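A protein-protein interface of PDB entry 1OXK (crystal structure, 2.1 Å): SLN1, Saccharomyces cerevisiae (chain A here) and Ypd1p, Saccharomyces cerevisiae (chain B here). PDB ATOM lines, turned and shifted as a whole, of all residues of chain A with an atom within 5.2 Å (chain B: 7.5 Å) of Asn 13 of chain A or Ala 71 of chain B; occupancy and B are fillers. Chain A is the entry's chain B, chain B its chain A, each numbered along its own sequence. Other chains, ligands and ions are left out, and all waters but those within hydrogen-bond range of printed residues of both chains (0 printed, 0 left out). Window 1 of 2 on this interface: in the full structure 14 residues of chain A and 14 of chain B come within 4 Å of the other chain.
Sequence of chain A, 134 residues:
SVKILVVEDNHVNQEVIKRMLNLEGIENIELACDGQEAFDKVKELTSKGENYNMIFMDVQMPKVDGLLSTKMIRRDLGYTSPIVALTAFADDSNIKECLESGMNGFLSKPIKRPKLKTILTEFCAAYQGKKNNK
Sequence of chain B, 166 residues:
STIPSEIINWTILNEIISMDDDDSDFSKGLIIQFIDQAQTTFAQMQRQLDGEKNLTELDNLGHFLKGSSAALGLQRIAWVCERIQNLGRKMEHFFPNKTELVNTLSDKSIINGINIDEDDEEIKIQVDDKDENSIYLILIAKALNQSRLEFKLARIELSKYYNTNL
OD1 of Asn 10 of chain A sits at hydrogen-bond distance from NE2 of Gln 37 of chain B, 2.8 Å away.
The side-chain amide nitrogen (ND2) of Asn 10 of chain A lies within hydrogen-bond range of the backbone carbonyl oxygen (O) of Phe 64 of chain B (2.8 Å).
The backbone carbonyl oxygen of Gly 67 of chain B sits at hydrogen-bond distance from the side-chain amide nitrogen of Asn 13 of chain A, 3.1 Å away.
OG of Ser 68 of chain B lies within hydrogen-bond range of OD1 of Asn 10 of chain A, 2.7 Å away.
N of Ile 12 of chain B is in hydrogen-bond range of OD1 of Asn 9 of chain B (3.5 Å).
The side-chain hydroxyl (OG) of Ser 68 of chain B lies within hydrogen-bond range of the side-chain amide oxygen (OE1) of Gln 37 of chain B (3.0 Å).
The side-chain amide oxygen of Asn 10 of chain A sits at hydrogen-bond distance from the backbone NH of Val 12 of chain A.
A ring nitrogen (ND1) of His 11 of chain A sits at hydrogen-bond distance from the side-chain amide oxygen (OE1) of Gln 14 of chain A (3.0 Å).
Among the printed residues, pairs that only touch across the chains: His 11 of chain A with Gln 33 of chain B (3.3 Å), Val 12 of chain A with Leu 30 of chain B (3.8 Å), Val 12 of chain A with Gln 33 of chain B (3.7 Å), Val 12 of chain A with Gln 37 of chain B (3.5 Å), Val 12 of chain A with Ser 68 of chain B (3.1 Å), Asn 13 of chain A with Ser 68 of chain B (3.6 Å), Asn 13 of chain A with Ala 71 of chain B (3.6 Å), Glu 15 of chain A with Leu 30 of chain B (3.8 Å), Glu 15 of chain A with Gln 33 of chain B (3.7 Å), Val 16 of chain A with Leu 30 of chain B (3.5 Å) and Pro 110 of chain A with Ile 12 of chain B (3.9 Å).
Glu 8 of chain A touches none of the printed residues of chain B.
Asn 13 of chain A touches just these residues of chain B: Gly 67 (3.1 Å), Ser 68 (3.6 Å) and Ala 71 (3.6 Å).
Printed residues of chain B within 4 Å of Glu 15 of chain A: Leu 30 (3.8 Å) and Gln 33 (3.7 Å).
Printed residues of chain A within 4 Å of Ile 12 of chain B: Pro 110.
Printed residues of chain A within 4 Å of Ser 68 of chain B: Asn 10, Val 12 and Asn 13.
Ser 69 of chain B touches none of the printed residues of chain A.
Printed residues of chain A within 4 Å of Ala 71 of chain B: Asn 13 (3.6 Å).
The nearest printed residue of chain B that does not touch Asn 13 of chain A is Phe 64 of chain B (5.8 Å).
The nearest printed residue of chain A that does not touch Phe 64 of chain B is His 11 of chain A (5.0 Å).
Of the 11 printed residues of chain A, 7 touch a printed residue of chain B.
Printed residues of chain A that touch a printed residue of chain B: Asn 10, His 11, Val 12, Asn 13, Glu 15, Val 16 and Pro 110.
Of the 22 printed residues of chain B, 8 touch a printed residue of chain A.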
ATOM      1  N   GLU A   8     -16.110  29.601   3.955  1.00  0.00           N
ATOM      2  CA  GLU A   8     -14.891  30.317   3.596  1.00  0.00           C
ATOM      3  C   GLU A   8     -14.944  30.648   2.098  1.00  0.00           C
ATOM      4  O   GLU A   8     -15.353  29.815   1.302  1.00  0.00           O
ATOM      5  CB  GLU A   8     -13.712  29.447   3.895  1.00  0.00           C
ATOM      6  CG  GLU A   8     -13.058  29.730   5.226  1.00  0.00           C
ATOM      7  CD  GLU A   8     -11.946  30.746   5.081  1.00  0.00           C
ATOM      8  OE1 GLU A   8     -11.831  31.393   3.992  1.00  0.00           O
ATOM      9  OE2 GLU A   8     -11.192  30.872   6.054  1.00  0.00           O
ATOM     10  N   ASN A  10     -12.681  30.946  -0.020  1.00  0.00           N
ATOM     11  CA  ASN A  10     -11.609  30.356  -0.783  1.00  0.00           C
ATOM     12  C   ASN A  10     -11.524  28.866  -0.491  1.00  0.00           C
ATOM     13  O   ASN A  10     -11.463  28.451   0.657  1.00  0.00           O
ATOM     14  CB  ASN A  10     -10.282  31.068  -0.502  1.00  0.00           C
ATOM     15  CG  ASN A  10      -9.204  30.679  -1.499  1.00  0.00           C
ATOM     16  OD1 ASN A  10      -8.848  29.485  -1.627  1.00  0.00           O
ATOM     17  ND2 ASN A  10      -8.669  31.684  -2.196  1.00  0.00           N
ATOM     18  N   HIS A  11     -11.590  28.067  -1.549  1.00  0.00           N
ATOM     19  CA  HIS A  11     -11.535  26.612  -1.468  1.00  0.00           C
ATOM     20  C   HIS A  11     -10.312  26.129  -0.712  1.00  0.00           C
ATOM     21  O   HIS A  11     -10.380  25.139   0.015  1.00  0.00           O
ATOM     22  CB  HIS A  11     -11.516  25.981  -2.872  1.00  0.00           C
ATOM     23  CG  HIS A  11     -12.828  26.012  -3.601  1.00  0.00           C
ATOM     24  ND1 HIS A  11     -14.025  25.657  -3.024  1.00  0.00           N
ATOM     25  CD2 HIS A  11     -13.122  26.332  -4.897  1.00  0.00           C
ATOM     26  CE1 HIS A  11     -14.995  25.744  -3.924  1.00  0.00           C
ATOM     27  NE2 HIS A  11     -14.476  26.166  -5.065  1.00  0.00           N
ATOM     28  N   VAL A  12      -9.177  26.788  -0.927  1.00  0.00           N
ATOM     29  CA  VAL A  12      -7.980  26.356  -0.265  1.00  0.00           C
ATOM     30  C   VAL A  12      -8.170  26.446   1.230  1.00  0.00           C
ATOM     31  O   VAL A  12      -7.900  25.466   1.927  1.00  0.00           O
ATOM     32  CB  VAL A  12      -6.770  27.121  -0.699  1.00  0.00           C
ATOM     33  CG1 VAL A  12      -5.634  26.935   0.303  1.00  0.00           C
ATOM     34  CG2 VAL A  12      -6.359  26.635  -2.074  1.00  0.00           C
ATOM     35  N   ASN A  13      -8.677  27.588   1.710  1.00  0.00           N
ATOM     36  CA  ASN A  13      -8.871  27.764   3.141  1.00  0.00           C
ATOM     37  C   ASN A  13      -9.871  26.727   3.666  1.00  0.00           C
ATOM     38  O   ASN A  13      -9.728  26.208   4.753  1.00  0.00           O
ATOM     39  CB  ASN A  13      -9.338  29.196   3.434  1.00  0.00           C
ATOM     40  CG  ASN A  13      -8.326  30.265   2.911  1.00  0.00           C
ATOM     41  OD1 ASN A  13      -7.991  30.298   1.734  1.00  0.00           O
ATOM     42  ND2 ASN A  13      -7.817  31.065   3.806  1.00  0.00           N
ATOM     43  N   GLN A  14     -10.890  26.457   2.877  1.00  0.00           N
ATOM     44  CA  GLN A  14     -11.905  25.477   3.247  1.00  0.00           C
ATOM     45  C   GLN A  14     -11.285  24.122   3.497  1.00  0.00           C
ATOM     46  O   GLN A  14     -11.650  23.429   4.483  1.00  0.00           O
ATOM     47  CB  GLN A  14     -12.909  25.315   2.131  1.00  0.00           C
ATOM     48  CG  GLN A  14     -13.839  26.472   1.881  1.00  0.00           C
ATOM     49  CD  GLN A  14     -14.783  26.162   0.734  1.00  0.00           C
ATOM     50  OE1 GLN A  14     -14.509  25.253  -0.077  1.00  0.00           O
ATOM     51  NE2 GLN A  14     -15.851  26.922   0.625  1.00  0.00           N
ATOM     52  N   GLU A  15     -10.375  23.718   2.600  1.00  0.00           N
ATOM     53  CA  GLU A  15      -9.724  22.402   2.715  1.00  0.00           C
ATOM     54  C   GLU A  15      -8.791  22.331   3.916  1.00  0.00           C
ATOM     55  O   GLU A  15      -8.572  21.250   4.496  1.00  0.00           O
ATOM     56  CB  GLU A  15      -8.919  22.046   1.454  1.00  0.00           C
ATOM     57  CG  GLU A  15      -9.715  21.731   0.206  1.00  0.00           C
ATOM     58  CD  GLU A  15     -10.619  20.510   0.365  1.00  0.00           C
ATOM     59  OE1 GLU A  15     -11.725  20.516  -0.222  1.00  0.00           O
ATOM     60  OE2 GLU A  15     -10.248  19.572   1.074  1.00  0.00           O
ATOM     61  N   VAL A  16      -8.187  23.453   4.268  1.00  0.00           N
ATOM     62  CA  VAL A  16      -7.325  23.451   5.448  1.00  0.00           C
ATOM     63  C   VAL A  16      -8.182  23.108   6.658  1.00  0.00           C
ATOM     64  O   VAL A  16      -7.816  22.228   7.442  1.00  0.00           O
ATOM     65  CB  VAL A  16      -6.623  24.798   5.638  1.00  0.00           C
ATOM     66  CG1 VAL A  16      -5.922  24.897   6.996  1.00  0.00           C
ATOM     67  CG2 VAL A  16      -5.622  25.009   4.552  1.00  0.00           C
ATOM     68  N   ILE A  17      -9.340  23.762   6.793  1.00  0.00           N
ATOM     69  CA  ILE A  17     -10.204  23.560   7.965  1.00  0.00           C
ATOM     70  C   ILE A  17     -10.863  22.179   7.961  1.00  0.00           C
ATOM     71  O   ILE A  17     -11.003  21.546   8.998  1.00  0.00           O
ATOM     72  CB  ILE A  17     -11.282  24.664   8.082  1.00  0.00           C
ATOM     73  CG1 ILE A  17     -10.602  25.998   8.375  1.00  0.00           C
ATOM     74  CG2 ILE A  17     -12.207  24.362   9.232  1.00  0.00           C
ATOM     75  CD1 ILE A  17     -11.413  27.221   8.025  1.00  0.00           C
ATOM     76  N   LYS A  18     -11.258  21.709   6.785  1.00  0.00           N
ATOM     77  CA  LYS A  18     -11.851  20.383   6.667  1.00  0.00           C
ATOM     78  C   LYS A  18     -10.868  19.321   7.151  1.00  0.00           C
ATOM     79  O   LYS A  18     -11.240  18.403   7.879  1.00  0.00           O
ATOM     80  CB  LYS A  18     -12.192  20.099   5.199  1.00  0.00           C
ATOM     81  CG  LYS A  18     -12.714  18.719   4.943  1.00  0.00           C
ATOM     82  CD  LYS A  18     -13.277  18.608   3.528  1.00  0.00           C
ATOM     83  CE  LYS A  18     -13.533  17.145   3.103  1.00  0.00           C
ATOM     84  NZ  LYS A  18     -14.373  17.040   1.837  1.00  0.00           N
ATOM     85  N   PRO A 110      -3.978  32.796  10.608  1.00  0.00           N
ATOM     86  CA  PRO A 110      -4.160  31.436  10.117  1.00  0.00           C
ATOM     87  C   PRO A 110      -4.609  30.543  11.224  1.00  0.00           C
ATOM     88  O   PRO A 110      -4.070  30.631  12.326  1.00  0.00           O
ATOM     89  CB  PRO A 110      -2.745  31.026   9.694  1.00  0.00           C
ATOM     90  CG  PRO A 110      -1.825  31.845  10.540  1.00  0.00           C
ATOM     91  CD  PRO A 110      -2.550  33.132  10.784  1.00  0.00           C
ATOM     92  N   ASN B   9       6.611  31.817   5.062  1.00  0.00           N
ATOM     93  CA  ASN B   9       6.527  31.870   6.517  1.00  0.00           C
ATOM     94  C   ASN B   9       6.346  30.395   6.994  1.00  0.00           C
ATOM     95  O   ASN B   9       5.229  29.832   6.973  1.00  0.00           O
ATOM     96  CB  ASN B   9       5.315  32.715   6.927  1.00  0.00           C
ATOM     97  CG  ASN B   9       5.206  32.950   8.426  1.00  0.00           C
ATOM     98  OD1 ASN B   9       5.784  32.257   9.240  1.00  0.00           O
ATOM     99  ND2 ASN B   9       4.475  33.995   8.777  1.00  0.00           N
ATOM    100  N   ILE B  12       3.762  29.467   9.570  1.00  0.00           N
ATOM    101  CA  ILE B  12       2.427  29.171   9.076  1.00  0.00           C
ATOM    102  C   ILE B  12       2.337  27.835   8.311  1.00  0.00           C
ATOM    103  O   ILE B  12       1.424  27.026   8.556  1.00  0.00           O
ATOM    104  CB  ILE B  12       1.928  30.317   8.179  1.00  0.00           C
ATOM    105  CG1 ILE B  12       1.711  31.584   9.017  1.00  0.00           C
ATOM    106  CG2 ILE B  12       0.616  29.934   7.518  1.00  0.00           C
ATOM    107  CD1 ILE B  12       1.362  32.851   8.158  1.00  0.00           C
ATOM    108  N   LEU B  13       3.254  27.607   7.370  1.00  0.00           N
ATOM    109  CA  LEU B  13       3.167  26.383   6.521  1.00  0.00           C
ATOM    110  C   LEU B  13       3.339  25.111   7.326  1.00  0.00           C
ATOM    111  O   LEU B  13       2.670  24.110   7.052  1.00  0.00           O
ATOM    112  CB  LEU B  13       4.171  26.427   5.382  1.00  0.00           C
ATOM    113  CG  LEU B  13       4.066  25.350   4.285  1.00  0.00           C
ATOM    114  CD1 LEU B  13       2.672  25.293   3.680  1.00  0.00           C
ATOM    115  CD2 LEU B  13       5.026  25.659   3.191  1.00  0.00           C
ATOM    116  N   GLU B  15       2.166  24.390  10.113  1.00  0.00           N
ATOM    117  CA  GLU B  15       0.871  23.940  10.658  1.00  0.00           C
ATOM    118  C   GLU B  15       0.149  23.031   9.674  1.00  0.00           C
ATOM    119  O   GLU B  15      -0.507  22.039  10.024  1.00  0.00           O
ATOM    120  CB  GLU B  15      -0.081  25.115  10.951  1.00  0.00           C
ATOM    121  CG  GLU B  15       0.022  25.686  12.360  1.00  0.00           C
ATOM    122  CD  GLU B  15      -0.440  24.708  13.423  1.00  0.00           C
ATOM    123  OE1 GLU B  15      -1.685  24.584  13.586  1.00  0.00           O
ATOM    124  OE2 GLU B  15       0.443  24.067  14.088  1.00  0.00           O
ATOM    125  N   ILE B  16       0.221  23.405   8.421  1.00  0.00           N
ATOM    126  CA  ILE B  16      -0.425  22.632   7.409  1.00  0.00           C
ATOM    127  C   ILE B  16       0.293  21.306   7.243  1.00  0.00           C
ATOM    128  O   ILE B  16      -0.364  20.274   7.209  1.00  0.00           O
ATOM    129  CB  ILE B  16      -0.471  23.434   6.118  1.00  0.00           C
ATOM    130  CG1 ILE B  16      -1.453  24.604   6.318  1.00  0.00           C
ATOM    131  CG2 ILE B  16      -0.945  22.548   4.992  1.00  0.00           C
ATOM    132  CD1 ILE B  16      -1.403  25.589   5.241  1.00  0.00           C
ATOM    133  N   LEU B  30      -2.752  20.327  -1.420  1.00  0.00           N
ATOM    134  CA  LEU B  30      -3.183  21.672  -1.125  1.00  0.00           C
ATOM    135  C   LEU B  30      -2.345  22.699  -1.876  1.00  0.00           C
ATOM    136  O   LEU B  30      -2.899  23.644  -2.402  1.00  0.00           O
ATOM    137  CB  LEU B  30      -3.078  21.940   0.373  1.00  0.00           C
ATOM    138  CG  LEU B  30      -3.830  23.177   0.887  1.00  0.00           C
ATOM    139  CD1 LEU B  30      -5.310  22.958   0.706  1.00  0.00           C
ATOM    140  CD2 LEU B  30      -3.492  23.433   2.339  1.00  0.00           C
ATOM    141  N   GLN B  33      -3.410  22.704  -5.450  1.00  0.00           N
ATOM    142  CA  GLN B  33      -4.664  23.414  -5.624  1.00  0.00           C
ATOM    143  C   GLN B  33      -4.347  24.918  -5.690  1.00  0.00           C
ATOM    144  O   GLN B  33      -4.843  25.642  -6.544  1.00  0.00           O
ATOM    145  CB  GLN B  33      -5.598  23.063  -4.471  1.00  0.00           C
ATOM    146  CG  GLN B  33      -7.008  23.603  -4.580  1.00  0.00           C
ATOM    147  CD  GLN B  33      -7.860  23.193  -3.406  1.00  0.00           C
ATOM    148  OE1 GLN B  33      -7.541  22.246  -2.724  1.00  0.00           O
ATOM    149  NE2 GLN B  33      -8.942  23.900  -3.178  1.00  0.00           N
ATOM    150  N   PHE B  34      -3.473  25.349  -4.781  1.00  0.00           N
ATOM    151  CA  PHE B  34      -3.118  26.735  -4.713  1.00  0.00           C
ATOM    152  C   PHE B  34      -2.551  27.172  -6.033  1.00  0.00           C
ATOM    153  O   PHE B  34      -2.982  28.190  -6.540  1.00  0.00           O
ATOM    154  CB  PHE B  34      -2.102  27.071  -3.620  1.00  0.00           C
ATOM    155  CG  PHE B  34      -1.645  28.453  -3.716  1.00  0.00           C
ATOM    156  CD1 PHE B  34      -2.491  29.487  -3.336  1.00  0.00           C
ATOM    157  CD2 PHE B  34      -0.436  28.762  -4.287  1.00  0.00           C
ATOM    158  CE1 PHE B  34      -2.110  30.740  -3.468  1.00  0.00           C
ATOM    159  CE2 PHE B  34      -0.071  30.026  -4.402  1.00  0.00           C
ATOM    160  CZ  PHE B  34      -0.892  31.014  -4.019  1.00  0.00           C
ATOM    161  N   GLN B  37      -5.114  27.618  -8.585  1.00  0.00           N
ATOM    162  CA  GLN B  37      -5.957  28.774  -8.270  1.00  0.00           C
ATOM    163  C   GLN B  37      -5.245  30.081  -8.603  1.00  0.00           C
ATOM    164  O   GLN B  37      -5.865  31.006  -9.167  1.00  0.00           O
ATOM    165  CB  GLN B  37      -6.426  28.678  -6.830  1.00  0.00           C
ATOM    166  CG  GLN B  37      -7.432  29.722  -6.457  1.00  0.00           C
ATOM    167  CD  GLN B  37      -7.466  29.895  -4.960  1.00  0.00           C
ATOM    168  OE1 GLN B  37      -6.921  30.877  -4.485  1.00  0.00           O
ATOM    169  NE2 GLN B  37      -7.982  28.907  -4.220  1.00  0.00           N
ATOM    170  N   PHE B  64      -9.391  37.476  -3.096  1.00  0.00           N
ATOM    171  CA  PHE B  64      -9.451  36.016  -3.184  1.00  0.00           C
ATOM    172  C   PHE B  64      -8.092  35.317  -3.104  1.00  0.00           C
ATOM    173  O   PHE B  64      -7.894  34.379  -2.363  1.00  0.00           O
ATOM    174  CB  PHE B  64     -10.127  35.697  -4.535  1.00  0.00           C
ATOM    175  CG  PHE B  64     -10.218  34.271  -4.861  1.00  0.00           C
ATOM    176  CD1 PHE B  64     -11.131  33.439  -4.181  1.00  0.00           C
ATOM    177  CD2 PHE B  64      -9.444  33.723  -5.904  1.00  0.00           C
ATOM    178  CE1 PHE B  64     -11.255  32.121  -4.502  1.00  0.00           C
ATOM    179  CE2 PHE B  64      -9.580  32.349  -6.233  1.00  0.00           C
ATOM    180  CZ  PHE B  64     -10.506  31.557  -5.501  1.00  0.00           C
ATOM    181  N   LEU B  65      -7.115  35.773  -3.858  1.00  0.00           N
ATOM    182  CA  LEU B  65      -5.806  35.128  -3.842  1.00  0.00           C
ATOM    183  C   LEU B  65      -5.019  35.432  -2.540  1.00  0.00           C
ATOM    184  O   LEU B  65      -4.165  34.647  -2.098  1.00  0.00           O
ATOM    185  CB  LEU B  65      -4.983  35.557  -5.019  1.00  0.00           C
ATOM    186  CG  LEU B  65      -3.790  34.650  -5.236  1.00  0.00           C
ATOM    187  CD1 LEU B  65      -4.127  33.154  -5.404  1.00  0.00           C
ATOM    188  CD2 LEU B  65      -3.096  35.130  -6.449  1.00  0.00           C
ATOM    189  N   LYS B  66      -5.277  36.591  -1.970  1.00  0.00           N
ATOM    190  CA  LYS B  66      -4.662  36.966  -0.732  1.00  0.00           C
ATOM    191  C   LYS B  66      -4.979  35.912   0.323  1.00  0.00           C
ATOM    192  O   LYS B  66      -4.085  35.467   1.013  1.00  0.00           O
ATOM    193  CB  LYS B  66      -5.146  38.366  -0.263  1.00  0.00           C
ATOM    194  CG  LYS B  66      -4.435  38.896   0.983  1.00  0.00           C
ATOM    195  CD  LYS B  66      -4.806  40.363   1.321  1.00  0.00           C
ATOM    196  CE  LYS B  66      -6.230  40.481   1.872  1.00  0.00           C
ATOM    197  NZ  LYS B  66      -6.625  41.945   2.187  1.00  0.00           N
ATOM    198  N   GLY B  67      -6.254  35.518   0.415  1.00  0.00           N
ATOM    199  CA  GLY B  67      -6.712  34.637   1.470  1.00  0.00           C
ATOM    200  C   GLY B  67      -6.015  33.294   1.444  1.00  0.00           C
ATOM    201  O   GLY B  67      -5.605  32.794   2.478  1.00  0.00           O
ATOM    202  N   SER B  68      -5.851  32.763   0.227  1.00  0.00           N
ATOM    203  CA  SER B  68      -5.162  31.487  -0.057  1.00  0.00           C
ATOM    204  C   SER B  68      -3.646  31.483   0.192  1.00  0.00           C
ATOM    205  O   SER B  68      -3.106  30.639   0.923  1.00  0.00           O
ATOM    206  CB  SER B  68      -5.376  31.151  -1.566  1.00  0.00           C
ATOM    207  OG  SER B  68      -6.203  30.030  -1.653  1.00  0.00           O
ATOM    208  N   SER B  69      -3.004  32.471  -0.411  1.00  0.00           N
ATOM    209  CA  SER B  69      -1.582  32.669  -0.286  1.00  0.00           C
ATOM    210  C   SER B  69      -1.241  32.930   1.197  1.00  0.00           C
ATOM    211  O   SER B  69      -0.339  32.299   1.756  1.00  0.00           O
ATOM    212  CB  SER B  69      -1.117  33.779  -1.193  1.00  0.00           C
ATOM    213  OG  SER B  69      -1.739  34.980  -0.889  1.00  0.00           O
ATOM    214  N   ALA B  70      -1.974  33.818   1.865  1.00  0.00           N
ATOM    215  CA  ALA B  70      -1.674  34.054   3.282  1.00  0.00           C
ATOM    216  C   ALA B  70      -1.751  32.770   4.098  1.00  0.00           C
ATOM    217  O   ALA B  70      -0.917  32.530   4.988  1.00  0.00           O
ATOM    218  CB  ALA B  70      -2.625  35.126   3.865  1.00  0.00           C
ATOM    219  N   ALA B  71      -2.769  31.952   3.835  1.00  0.00           N
ATOM    220  CA  ALA B  71      -3.001  30.742   4.618  1.00  0.00           C
ATOM    221  C   ALA B  71      -1.925  29.674   4.472  1.00  0.00           C
ATOM    222  O   ALA B  71      -1.764  28.831   5.354  1.00  0.00           O
ATOM    223  CB  ALA B  71      -4.369  30.167   4.253  1.00  0.00           C
ATOM    224  N   LEU B  72      -1.223  29.701   3.346  1.00  0.00           N
ATOM    225  CA  LEU B  72      -0.138  28.783   3.070  1.00  0.00           C
ATOM    226  C   LEU B  72       1.168  29.393   3.459  1.00  0.00           C
ATOM    227  O   LEU B  72       2.191  28.742   3.341  1.00  0.00           O
ATOM    228  CB  LEU B  72      -0.092  28.386   1.580  1.00  0.00           C
ATOM    229  CG  LEU B  72      -1.284  27.542   1.137  1.00  0.00           C
ATOM    230  CD1 LEU B  72      -1.267  27.331  -0.326  1.00  0.00           C
ATOM    231  CD2 LEU B  72      -1.317  26.244   1.847  1.00  0.00           C
ATOM    232  N   GLY B  73       1.159  30.642   3.932  1.00  0.00           N
ATOM    233  CA  GLY B  73       2.390  31.280   4.329  1.00  0.00           C
ATOM    234  C   GLY B  73       3.183  31.895   3.174  1.00  0.00           C
ATOM    235  O   GLY B  73       4.323  32.293   3.363  1.00  0.00           O
ATOM    236  N   LEU B  74       2.574  31.979   1.993  1.00  0.00           N
ATOM    237  CA  LEU B  74       3.241  32.544   0.824  1.00  0.00           C
ATOM    238  C   LEU B  74       2.991  34.068   0.973  1.00  0.00           C
ATOM    239  O   LEU B  74       2.207  34.698   0.253  1.00  0.00           O
ATOM    240  CB  LEU B  74       2.678  31.936  -0.468  1.00  0.00           C
ATOM    241  CG  LEU B  74       2.613  30.400  -0.328  1.00  0.00           C
ATOM    242  CD1 LEU B  74       2.017  29.726  -1.589  1.00  0.00           C
ATOM    243  CD2 LEU B  74       3.985  29.826  -0.028  1.00  0.00           C
ATOM    244  N   GLN B  75       3.720  34.636   1.906  1.00  0.00           N
ATOM    245  CA  GLN B  75       3.413  35.967   2.382  1.00  0.00           C
ATOM    246  C   GLN B  75       3.847  37.065   1.437  1.00  0.00           C
ATOM    247  O   GLN B  75       3.314  38.162   1.512  1.00  0.00           O
ATOM    248  CB  GLN B  75       4.032  36.157   3.782  1.00  0.00           C
ATOM    249  CG  GLN B  75       5.559  35.950   3.773  1.00  0.00           C
ATOM    250  CD  GLN B  75       6.172  36.020   5.182  1.00  0.00           C
ATOM    251  OE1 GLN B  75       5.452  36.232   6.128  1.00  0.00           O
ATOM    252  NE2 GLN B  75       7.495  35.842   5.291  1.00  0.00           N
ATOM    253  N   ALA B  78       1.021  37.253  -0.899  1.00  0.00           N
ATOM    254  CA  ALA B  78      -0.133  37.816  -0.187  1.00  0.00           C
ATOM    255  C   ALA B  78      -0.010  39.368  -0.144  1.00  0.00           C
ATOM    256  O   ALA B  78      -0.972  40.082  -0.381  1.00  0.00           O
ATOM    257  CB  ALA B  78      -0.241  37.208   1.205  1.00  0.00           C
